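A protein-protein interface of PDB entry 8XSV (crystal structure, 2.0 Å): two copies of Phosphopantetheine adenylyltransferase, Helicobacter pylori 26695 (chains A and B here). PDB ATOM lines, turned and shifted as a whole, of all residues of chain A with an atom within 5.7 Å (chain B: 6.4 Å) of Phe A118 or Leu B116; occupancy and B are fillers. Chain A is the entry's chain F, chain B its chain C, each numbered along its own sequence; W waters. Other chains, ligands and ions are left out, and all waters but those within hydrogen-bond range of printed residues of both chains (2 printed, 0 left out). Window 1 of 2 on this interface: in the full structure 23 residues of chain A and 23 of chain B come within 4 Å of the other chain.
The backbone carbonyl oxygen of Leu B116 lies within hydrogen-bond range of the backbone NH of Arg B88, 2.8 Å away.
O of Arg B88 sits at hydrogen-bond distance from N of Phe B118, at 3.0 Å.
The guanidinium group (NE) of Arg A24 sits close to the backbone carbonyl oxygen (O) of Met A119 (3.1 Å).
The backbone NH (N) of Arg A88 is in hydrogen-bond range of the backbone carbonyl oxygen (O) of Leu A116, 2.8 Å away.
The backbone carbonyl oxygen (O) of Arg A88 sits at hydrogen-bond distance from the backbone NH (N) of Phe A118 (2.9 Å).
The backbone carbonyl oxygen (O) of Phe A118 lies within hydrogen-bond range of the backbone NH (N) of Leu A90, at 2.7 Å.
Leu A28 touches its own counterpart, Leu B28.
Leu A116 touches Tyr B117, and with the chains exchanged Tyr A117 touches Leu B116.
Leu A116 touches Phe B118, and with the chains exchanged Phe A118 touches Leu B116.
Tyr A117 touches its own counterpart, Tyr B117.
Of the 10 pairs that touch across the chains among the printed residues, 6 have their exchanged pair printed and touching as well.
Of the 15 printed residues of chain A, 7 touch a printed residue of chain B.
Printed residues of chain A that touch a printed residue of chain B: Arg A24, Leu A28, Arg A91, Leu A116, Tyr A117, Phe A118 and Met A119.
Hydrophobic or aromatic side chains of chain A that line the printed part of chain B: Leu A28, Leu A116, Tyr A117, Phe A118 and Met A119.
Hydrophobic or aromatic side chains of chain B within 4 Å of the printed part of chain A: Leu B28, Leu B100, Leu B116, Tyr B117 and Phe B118.
Among the printed residues, 10 pairs touch across the chains.
Among the printed residues, Asp or Glu carboxylates within 4 Å of a Lys or Arg side-chain nitrogen of the other chain: Arg A24 with Glu B114.
Water W1 bridges the guanidinium group (NH2) of Arg A24 (2.6 Å) and the side-chain carboxylate (OE2) of Glu B114 (2.9 Å).
Water W2 lies within hydrogen-bond range of the backbone carbonyl oxygen (O) of Thr B115 and the backbone NH (N) of Met A119.
Phe A118 touches just one residue of chain B: Leu B116 (3.4 Å).
Leu B116 touches two residues of chain A.
Of the printed residues of chain A, Phe B118 touches Leu A116 (3.7 Å).
Of the printed residues of chain A, Leu B28 touches Leu A28.
Printed residues of chain B within 4 Å of Arg A91: Leu B100.
The nearest residue of chain B that does not touch Phe A118 is Thr B115 (4.6 Å).
The nearest printed residue of chain B that does not touch Met A119 is Thr B115 (4.2 Å).
Leu B28 touches Leu A28.
Leu B100 touches Arg A91.
Tyr B117 touches Leu A116.
CG of Leu A116 touches CE1 of Phe B118, at 3.7 Å.
Tyr A117 touches Leu B116.
Leu B116 touches Phe A118 (CD1 to CZ, 3.4 Å).
CE of Met A119 touches O of Leu B100, 3.8 Å away.
OE1 of Glu B114 lies within salt-bridge range of NE of Arg A24 (3.8 Å).
The backbone NH (N) of Tyr A117 is in hydrogen-bond range of the backbone carbonyl oxygen (O) of Tyr B117 (2.9 Å).
The side-chain hydroxyl (OH) of Tyr B117 lies within hydrogen-bond range of the side-chain sulfur (SD) of Met A119 (3.6 Å).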
ATOM      1  N   ILE A  21     -12.233 -23.081 -24.889  1.00  0.00           N
ATOM      2  CA  ILE A  21     -12.687 -22.988 -23.510  1.00  0.00           C
ATOM      3  C   ILE A  21     -14.081 -22.308 -23.541  1.00  0.00           C
ATOM      4  O   ILE A  21     -14.968 -22.693 -22.784  1.00  0.00           O
ATOM      5  CB  ILE A  21     -11.682 -22.186 -22.630  1.00  0.00           C
ATOM      6  CG1 ILE A  21     -10.303 -22.960 -22.548  1.00  0.00           C
ATOM      7  CG2 ILE A  21     -12.235 -21.932 -21.252  1.00  0.00           C
ATOM      8  CD1 ILE A  21     -10.401 -24.368 -22.045  1.00  0.00           C
ATOM      9  N   ARG A  24     -16.518 -24.885 -24.706  1.00  0.00           N
ATOM     10  CA  ARG A  24     -16.804 -25.872 -23.642  1.00  0.00           C
ATOM     11  C   ARG A  24     -17.555 -25.403 -22.395  1.00  0.00           C
ATOM     12  O   ARG A  24     -18.528 -26.091 -21.920  1.00  0.00           O
ATOM     13  CB  ARG A  24     -15.502 -26.678 -23.325  1.00  0.00           C
ATOM     14  CG  ARG A  24     -15.213 -27.661 -24.467  1.00  0.00           C
ATOM     15  CD  ARG A  24     -13.727 -28.017 -24.471  1.00  0.00           C
ATOM     16  NE  ARG A  24     -13.103 -29.156 -25.221  1.00  0.00           N
ATOM     17  CZ  ARG A  24     -13.498 -29.746 -26.342  1.00  0.00           C
ATOM     18  NH1 ARG A  24     -12.746 -30.730 -26.813  1.00  0.00           N
ATOM     19  NH2 ARG A  24     -14.610 -29.382 -27.037  1.00  0.00           N
ATOM     20  N   SER A  25     -17.092 -24.290 -21.786  1.00  0.00           N
ATOM     21  CA  SER A  25     -17.758 -23.826 -20.551  1.00  0.00           C
ATOM     22  C   SER A  25     -19.143 -23.253 -20.896  1.00  0.00           C
ATOM     23  O   SER A  25     -20.030 -23.233 -20.066  1.00  0.00           O
ATOM     24  CB  SER A  25     -16.941 -22.706 -19.854  1.00  0.00           C
ATOM     25  OG  SER A  25     -16.692 -21.631 -20.767  1.00  0.00           O
ATOM     26  N   LEU A  28     -21.809 -25.656 -20.106  1.00  0.00           N
ATOM     27  CA  LEU A  28     -21.977 -26.040 -18.717  1.00  0.00           C
ATOM     28  C   LEU A  28     -22.744 -25.016 -17.818  1.00  0.00           C
ATOM     29  O   LEU A  28     -23.097 -25.337 -16.710  1.00  0.00           O
ATOM     30  CB  LEU A  28     -20.592 -26.405 -18.032  1.00  0.00           C
ATOM     31  CG  LEU A  28     -20.183 -27.926 -17.858  1.00  0.00           C
ATOM     32  CD1 LEU A  28     -21.313 -28.668 -17.077  1.00  0.00           C
ATOM     33  CD2 LEU A  28     -20.114 -28.475 -19.271  1.00  0.00           C
ATOM     34  N   PHE A  29     -22.948 -23.789 -18.294  1.00  0.00           N
ATOM     35  CA  PHE A  29     -23.712 -22.825 -17.553  1.00  0.00           C
ATOM     36  C   PHE A  29     -24.795 -22.196 -18.496  1.00  0.00           C
ATOM     37  O   PHE A  29     -24.550 -22.029 -19.684  1.00  0.00           O
ATOM     38  CB  PHE A  29     -22.783 -21.686 -16.986  1.00  0.00           C
ATOM     39  CG  PHE A  29     -21.534 -22.218 -16.315  1.00  0.00           C
ATOM     40  CD1 PHE A  29     -20.329 -22.329 -17.011  1.00  0.00           C
ATOM     41  CD2 PHE A  29     -21.597 -22.728 -15.033  1.00  0.00           C
ATOM     42  CE1 PHE A  29     -19.218 -22.936 -16.418  1.00  0.00           C
ATOM     43  CE2 PHE A  29     -20.523 -23.320 -14.430  1.00  0.00           C
ATOM     44  CZ  PHE A  29     -19.338 -23.409 -15.095  1.00  0.00           C
ATOM     45  N   VAL A  87     -14.375 -19.522 -14.574  1.00  0.00           N
ATOM     46  CA  VAL A  87     -13.957 -20.530 -15.495  1.00  0.00           C
ATOM     47  C   VAL A  87     -12.515 -20.297 -15.840  1.00  0.00           C
ATOM     48  O   VAL A  87     -12.110 -19.087 -16.125  1.00  0.00           O
ATOM     49  CB  VAL A  87     -14.799 -20.414 -16.787  1.00  0.00           C
ATOM     50  CG1 VAL A  87     -14.235 -21.403 -17.831  1.00  0.00           C
ATOM     51  CG2 VAL A  87     -16.268 -20.782 -16.479  1.00  0.00           C
ATOM     52  N   ARG A  88     -11.692 -21.340 -15.782  1.00  0.00           N
ATOM     53  CA  ARG A  88     -10.301 -21.172 -16.314  1.00  0.00           C
ATOM     54  C   ARG A  88     -10.011 -22.284 -17.288  1.00  0.00           C
ATOM     55  O   ARG A  88     -10.657 -23.353 -17.240  1.00  0.00           O
ATOM     56  CB  ARG A  88      -9.206 -21.307 -15.178  1.00  0.00           C
ATOM     57  CG  ARG A  88      -9.212 -20.268 -14.047  1.00  0.00           C
ATOM     58  CD  ARG A  88      -8.837 -18.897 -14.548  1.00  0.00           C
ATOM     59  NE  ARG A  88      -7.350 -18.897 -14.814  1.00  0.00           N
ATOM     60  CZ  ARG A  88      -6.717 -17.932 -15.452  1.00  0.00           C
ATOM     61  NH1 ARG A  88      -7.427 -16.943 -15.918  1.00  0.00           N
ATOM     62  NH2 ARG A  88      -5.375 -17.981 -15.614  1.00  0.00           N
ATOM     63  N   GLY A  89      -9.085 -22.064 -18.239  1.00  0.00           N
ATOM     64  CA  GLY A  89      -8.783 -23.234 -19.074  1.00  0.00           C
ATOM     65  C   GLY A  89      -7.479 -23.798 -18.585  1.00  0.00           C
ATOM     66  O   GLY A  89      -6.608 -23.029 -18.181  1.00  0.00           O
ATOM     67  N   LEU A  90      -7.293 -25.118 -18.635  1.00  0.00           N
ATOM     68  CA  LEU A  90      -5.990 -25.706 -18.325  1.00  0.00           C
ATOM     69  C   LEU A  90      -5.377 -26.251 -19.584  1.00  0.00           C
ATOM     70  O   LEU A  90      -6.046 -26.964 -20.379  1.00  0.00           O
ATOM     71  CB  LEU A  90      -6.144 -26.935 -17.474  1.00  0.00           C
ATOM     72  CG  LEU A  90      -6.426 -26.753 -16.026  1.00  0.00           C
ATOM     73  CD1 LEU A  90      -6.292 -28.196 -15.510  1.00  0.00           C
ATOM     74  CD2 LEU A  90      -5.387 -25.803 -15.438  1.00  0.00           C
ATOM     75  N   ARG A  91      -4.129 -25.855 -19.825  1.00  0.00           N
ATOM     76  CA  ARG A  91      -3.380 -26.353 -20.986  1.00  0.00           C
ATOM     77  C   ARG A  91      -2.004 -26.826 -20.558  1.00  0.00           C
ATOM     78  O   ARG A  91      -1.672 -26.862 -19.310  1.00  0.00           O
ATOM     79  CB  ARG A  91      -3.253 -25.257 -22.063  1.00  0.00           C
ATOM     80  CG  ARG A  91      -3.368 -23.814 -21.537  1.00  0.00           C
ATOM     81  CD  ARG A  91      -2.054 -23.331 -20.999  1.00  0.00           C
ATOM     82  NE  ARG A  91      -2.080 -21.876 -20.649  1.00  0.00           N
ATOM     83  CZ  ARG A  91      -1.720 -20.897 -21.471  1.00  0.00           C
ATOM     84  NH1 ARG A  91      -1.701 -19.614 -21.077  1.00  0.00           N
ATOM     85  NH2 ARG A  91      -1.379 -21.206 -22.694  1.00  0.00           N
ATOM     86  N   LEU A 116     -13.428 -23.257 -11.633  1.00  0.00           N
ATOM     87  CA  LEU A 116     -13.624 -24.523 -12.315  1.00  0.00           C
ATOM     88  C   LEU A 116     -12.774 -24.505 -13.600  1.00  0.00           C
ATOM     89  O   LEU A 116     -12.701 -23.460 -14.286  1.00  0.00           O
ATOM     90  CB  LEU A 116     -15.176 -24.661 -12.690  1.00  0.00           C
ATOM     91  CG  LEU A 116     -16.163 -25.222 -11.628  1.00  0.00           C
ATOM     92  CD1 LEU A 116     -16.082 -24.496 -10.250  1.00  0.00           C
ATOM     93  CD2 LEU A 116     -17.578 -25.206 -12.207  1.00  0.00           C
ATOM     94  N   TYR A 117     -12.190 -25.622 -13.968  1.00  0.00           N
ATOM     95  CA  TYR A 117     -11.204 -25.651 -15.042  1.00  0.00           C
ATOM     96  C   TYR A 117     -11.694 -26.557 -16.172  1.00  0.00           C
ATOM     97  O   TYR A 117     -12.094 -27.690 -15.874  1.00  0.00           O
ATOM     98  CB  TYR A 117      -9.831 -26.211 -14.483  1.00  0.00           C
ATOM     99  CG  TYR A 117      -9.258 -25.395 -13.366  1.00  0.00           C
ATOM    100  CD1 TYR A 117      -8.405 -24.337 -13.624  1.00  0.00           C
ATOM    101  CD2 TYR A 117      -9.681 -25.564 -12.089  1.00  0.00           C
ATOM    102  CE1 TYR A 117      -7.914 -23.537 -12.588  1.00  0.00           C
ATOM    103  CE2 TYR A 117      -9.163 -24.794 -11.021  1.00  0.00           C
ATOM    104  CZ  TYR A 117      -8.263 -23.806 -11.306  1.00  0.00           C
ATOM    105  OH  TYR A 117      -7.828 -22.988 -10.328  1.00  0.00           O
ATOM    106  N   PHE A 118     -11.652 -26.078 -17.386  1.00  0.00           N
ATOM    107  CA  PHE A 118     -11.932 -26.830 -18.608  1.00  0.00           C
ATOM    108  C   PHE A 118     -10.642 -27.065 -19.425  1.00  0.00           C
ATOM    109  O   PHE A 118      -9.627 -26.379 -19.172  1.00  0.00           O
ATOM    110  CB  PHE A 118     -12.931 -26.076 -19.489  1.00  0.00           C
ATOM    111  CG  PHE A 118     -14.298 -25.926 -18.809  1.00  0.00           C
ATOM    112  CD1 PHE A 118     -15.337 -26.655 -19.197  1.00  0.00           C
ATOM    113  CD2 PHE A 118     -14.455 -25.034 -17.759  1.00  0.00           C
ATOM    114  CE1 PHE A 118     -16.600 -26.539 -18.612  1.00  0.00           C
ATOM    115  CE2 PHE A 118     -15.658 -24.908 -17.124  1.00  0.00           C
ATOM    116  CZ  PHE A 118     -16.775 -25.652 -17.600  1.00  0.00           C
ATOM    117  N   MET A 119     -10.660 -28.050 -20.291  1.00  0.00           N
ATOM    118  CA  MET A 119      -9.544 -28.321 -21.152  1.00  0.00           C
ATOM    119  C   MET A 119      -9.996 -27.977 -22.597  1.00  0.00           C
ATOM    120  O   MET A 119     -11.086 -28.261 -22.974  1.00  0.00           O
ATOM    121  CB  MET A 119      -9.059 -29.794 -21.180  1.00  0.00           C
ATOM    122  CG  MET A 119      -9.022 -30.463 -19.777  1.00  0.00           C
ATOM    123  SD  MET A 119      -9.106 -32.241 -19.929  1.00  0.00           S
ATOM    124  CE  MET A 119      -8.151 -32.567 -21.367  1.00  0.00           C
ATOM    125  N   PRO A 120      -9.047 -27.475 -23.397  1.00  0.00           N
ATOM    126  CA  PRO A 120      -9.276 -27.229 -24.824  1.00  0.00           C
ATOM    127  C   PRO A 120      -9.166 -28.530 -25.577  1.00  0.00           C
ATOM    128  O   PRO A 120      -8.849 -29.569 -25.032  1.00  0.00           O
ATOM    129  CB  PRO A 120      -8.080 -26.263 -25.152  1.00  0.00           C
ATOM    130  CG  PRO A 120      -6.926 -26.819 -24.290  1.00  0.00           C
ATOM    131  CD  PRO A 120      -7.616 -27.292 -23.010  1.00  0.00           C
ATOM    132  N   LEU B  28     -23.443 -28.353  -9.178  1.00  0.00           N
ATOM    133  CA  LEU B  28     -23.565 -28.118 -10.592  1.00  0.00           C
ATOM    134  C   LEU B  28     -24.420 -29.150 -11.353  1.00  0.00           C
ATOM    135  O   LEU B  28     -25.099 -28.815 -12.378  1.00  0.00           O
ATOM    136  CB  LEU B  28     -22.153 -28.136 -11.195  1.00  0.00           C
ATOM    137  CG  LEU B  28     -22.149 -27.873 -12.714  1.00  0.00           C
ATOM    138  CD1 LEU B  28     -22.770 -26.460 -12.938  1.00  0.00           C
ATOM    139  CD2 LEU B  28     -20.722 -27.956 -13.250  1.00  0.00           C
ATOM    140  N   PHE B  29     -24.304 -30.411 -10.949  1.00  0.00           N
ATOM    141  CA  PHE B  29     -25.045 -31.463 -11.607  1.00  0.00           C
ATOM    142  C   PHE B  29     -26.353 -31.806 -10.848  1.00  0.00           C
ATOM    143  O   PHE B  29     -26.352 -31.817  -9.631  1.00  0.00           O
ATOM    144  CB  PHE B  29     -24.199 -32.672 -11.815  1.00  0.00           C
ATOM    145  CG  PHE B  29     -23.004 -32.372 -12.679  1.00  0.00           C
ATOM    146  CD1 PHE B  29     -21.763 -31.950 -12.063  1.00  0.00           C
ATOM    147  CD2 PHE B  29     -23.105 -32.394 -14.087  1.00  0.00           C
ATOM    148  CE1 PHE B  29     -20.662 -31.644 -12.840  1.00  0.00           C
ATOM    149  CE2 PHE B  29     -21.979 -32.058 -14.863  1.00  0.00           C
ATOM    150  CZ  PHE B  29     -20.756 -31.731 -14.215  1.00  0.00           C
ATOM    151  N   VAL B  85     -19.947 -35.542 -18.690  1.00  0.00           N
ATOM    152  CA  VAL B  85     -18.913 -34.883 -17.816  1.00  0.00           C
ATOM    153  C   VAL B  85     -18.339 -35.752 -16.724  1.00  0.00           C
ATOM    154  O   VAL B  85     -19.030 -36.173 -15.809  1.00  0.00           O
ATOM    155  CB  VAL B  85     -19.358 -33.553 -17.144  1.00  0.00           C
ATOM    156  CG1 VAL B  85     -18.128 -32.770 -16.577  1.00  0.00           C
ATOM    157  CG2 VAL B  85     -20.164 -32.676 -18.153  1.00  0.00           C
ATOM    158  N   LEU B  86     -17.001 -35.912 -16.765  1.00  0.00           N
ATOM    159  CA  LEU B  86     -16.224 -36.510 -15.653  1.00  0.00           C
ATOM    160  C   LEU B  86     -15.804 -35.363 -14.785  1.00  0.00           C
ATOM    161  O   LEU B  86     -15.365 -34.286 -15.290  1.00  0.00           O
ATOM    162  CB  LEU B  86     -15.022 -37.315 -16.156  1.00  0.00           C
ATOM    163  CG  LEU B  86     -15.351 -38.439 -17.173  1.00  0.00           C
ATOM    164  CD1 LEU B  86     -14.008 -39.129 -17.682  1.00  0.00           C
ATOM    165  CD2 LEU B  86     -16.340 -39.427 -16.481  1.00  0.00           C
ATOM    166  N   VAL B  87     -15.845 -35.595 -13.479  1.00  0.00           N
ATOM    167  CA  VAL B  87     -15.488 -34.569 -12.537  1.00  0.00           C
ATOM    168  C   VAL B  87     -14.137 -35.029 -11.969  1.00  0.00           C
ATOM    169  O   VAL B  87     -14.027 -36.152 -11.523  1.00  0.00           O
ATOM    170  CB  VAL B  87     -16.577 -34.519 -11.391  1.00  0.00           C
ATOM    171  CG1 VAL B  87     -16.090 -33.702 -10.151  1.00  0.00           C
ATOM    172  CG2 VAL B  87     -17.911 -33.898 -11.887  1.00  0.00           C
ATOM    173  N   ARG B  88     -13.157 -34.117 -11.853  1.00  0.00           N
ATOM    174  CA  ARG B  88     -11.913 -34.486 -11.159  1.00  0.00           C
ATOM    175  C   ARG B  88     -11.581 -33.383 -10.110  1.00  0.00           C
ATOM    176  O   ARG B  88     -12.104 -32.272 -10.181  1.00  0.00           O
ATOM    177  CB  ARG B  88     -10.731 -34.547 -12.186  1.00  0.00           C
ATOM    178  CG  ARG B  88     -10.857 -35.612 -13.228  1.00  0.00           C
ATOM    179  CD  ARG B  88     -10.655 -36.988 -12.646  1.00  0.00           C
ATOM    180  NE  ARG B  88      -9.229 -37.149 -12.225  1.00  0.00           N
ATOM    181  CZ  ARG B  88      -8.831 -38.193 -11.524  1.00  0.00           C
ATOM    182  NH1 ARG B  88      -9.739 -39.073 -11.164  1.00  0.00           N
ATOM    183  NH2 ARG B  88      -7.548 -38.367 -11.165  1.00  0.00           N
ATOM    184  N   GLY B  89     -10.820 -33.734  -9.079  1.00  0.00           N
ATOM    185  CA  GLY B  89     -10.424 -32.720  -8.141  1.00  0.00           C
ATOM    186  C   GLY B  89      -8.977 -32.370  -8.413  1.00  0.00           C
ATOM    187  O   GLY B  89      -8.168 -33.286  -8.689  1.00  0.00           O
ATOM    188  N   LEU B 100      -4.475 -34.080 -17.593  1.00  0.00           N
ATOM    189  CA  LEU B 100      -4.795 -33.719 -18.988  1.00  0.00           C
ATOM    190  C   LEU B 100      -4.729 -35.018 -19.863  1.00  0.00           C
ATOM    191  O   LEU B 100      -5.560 -35.220 -20.754  1.00  0.00           O
ATOM    192  CB  LEU B 100      -3.791 -32.748 -19.568  1.00  0.00           C
ATOM    193  CG  LEU B 100      -3.702 -31.311 -18.905  1.00  0.00           C
ATOM    194  CD1 LEU B 100      -2.698 -30.457 -19.645  1.00  0.00           C
ATOM    195  CD2 LEU B 100      -5.122 -30.639 -18.991  1.00  0.00           C
ATOM    196  N   GLU B 114     -16.514 -35.022 -21.601  1.00  0.00           N
ATOM    197  CA  GLU B 114     -15.661 -33.913 -21.176  1.00  0.00           C
ATOM    198  C   GLU B 114     -15.115 -34.211 -19.823  1.00  0.00           C
ATOM    199  O   GLU B 114     -15.662 -35.095 -19.061  1.00  0.00           O
ATOM    200  CB  GLU B 114     -16.516 -32.678 -21.032  1.00  0.00           C
ATOM    201  CG  GLU B 114     -17.282 -32.281 -22.316  1.00  0.00           C
ATOM    202  CD  GLU B 114     -16.340 -32.255 -23.577  1.00  0.00           C
ATOM    203  OE1 GLU B 114     -15.154 -31.860 -23.557  1.00  0.00           O
ATOM    204  OE2 GLU B 114     -16.856 -32.497 -24.636  1.00  0.00           O
ATOM    205  N   THR B 115     -14.027 -33.499 -19.475  1.00  0.00           N
ATOM    206  CA  THR B 115     -13.536 -33.564 -18.028  1.00  0.00           C
ATOM    207  C   THR B 115     -13.522 -32.174 -17.489  1.00  0.00           C
ATOM    208  O   THR B 115     -13.033 -31.261 -18.123  1.00  0.00           O
ATOM    209  CB  THR B 115     -12.139 -34.240 -17.887  1.00  0.00           C
ATOM    210  OG1 THR B 115     -12.175 -35.584 -18.413  1.00  0.00           O
ATOM    211  CG2 THR B 115     -11.671 -34.285 -16.452  1.00  0.00           C
ATOM    212  N   LEU B 116     -14.081 -31.987 -16.321  1.00  0.00           N
ATOM    213  CA  LEU B 116     -14.132 -30.736 -15.576  1.00  0.00           C
ATOM    214  C   LEU B 116     -13.462 -30.809 -14.233  1.00  0.00           C
ATOM    215  O   LEU B 116     -13.657 -31.878 -13.447  1.00  0.00           O
ATOM    216  CB  LEU B 116     -15.568 -30.446 -15.279  1.00  0.00           C
ATOM    217  CG  LEU B 116     -16.032 -29.196 -14.577  1.00  0.00           C
ATOM    218  CD1 LEU B 116     -15.606 -27.848 -15.225  1.00  0.00           C
ATOM    219  CD2 LEU B 116     -17.608 -29.205 -14.482  1.00  0.00           C
ATOM    220  N   TYR B 117     -12.748 -29.763 -13.854  1.00  0.00           N
ATOM    221  CA  TYR B 117     -12.002 -29.883 -12.591  1.00  0.00           C
ATOM    222  C   TYR B 117     -12.448 -28.868 -11.586  1.00  0.00           C
ATOM    223  O   TYR B 117     -12.605 -27.701 -11.996  1.00  0.00           O
ATOM    224  CB  TYR B 117     -10.449 -29.589 -12.874  1.00  0.00           C
ATOM    225  CG  TYR B 117      -9.852 -30.588 -13.899  1.00  0.00           C
ATOM    226  CD1 TYR B 117      -9.251 -31.746 -13.477  1.00  0.00           C
ATOM    227  CD2 TYR B 117      -9.856 -30.290 -15.253  1.00  0.00           C
ATOM    228  CE1 TYR B 117      -8.716 -32.661 -14.367  1.00  0.00           C
ATOM    229  CE2 TYR B 117      -9.303 -31.132 -16.153  1.00  0.00           C
ATOM    230  CZ  TYR B 117      -8.719 -32.330 -15.696  1.00  0.00           C
ATOM    231  OH  TYR B 117      -8.160 -33.190 -16.619  1.00  0.00           O
ATOM    232  N   PHE B 118     -12.615 -29.323 -10.307  1.00  0.00           N
ATOM    233  CA  PHE B 118     -12.863 -28.550  -9.121  1.00  0.00           C
ATOM    234  C   PHE B 118     -11.666 -28.457  -8.172  1.00  0.00           C
ATOM    235  O   PHE B 118     -10.762 -29.295  -8.248  1.00  0.00           O
ATOM    236  CB  PHE B 118     -14.047 -29.177  -8.357  1.00  0.00           C
ATOM    237  CG  PHE B 118     -15.396 -29.135  -9.193  1.00  0.00           C
ATOM    238  CD1 PHE B 118     -16.323 -28.128  -8.990  1.00  0.00           C
ATOM    239  CD2 PHE B 118     -15.551 -29.973 -10.244  1.00  0.00           C
ATOM    240  CE1 PHE B 118     -17.530 -28.083  -9.748  1.00  0.00           C
ATOM    241  CE2 PHE B 118     -16.711 -29.977 -11.011  1.00  0.00           C
ATOM    242  CZ  PHE B 118     -17.696 -29.024 -10.770  1.00  0.00           C
HETATM  243  O   HOH W   1     -16.916 -29.862 -25.954  1.00  0.00           O
HETATM  244  O   HOH W   2     -13.108 -29.623 -20.379  1.00  0.00           O
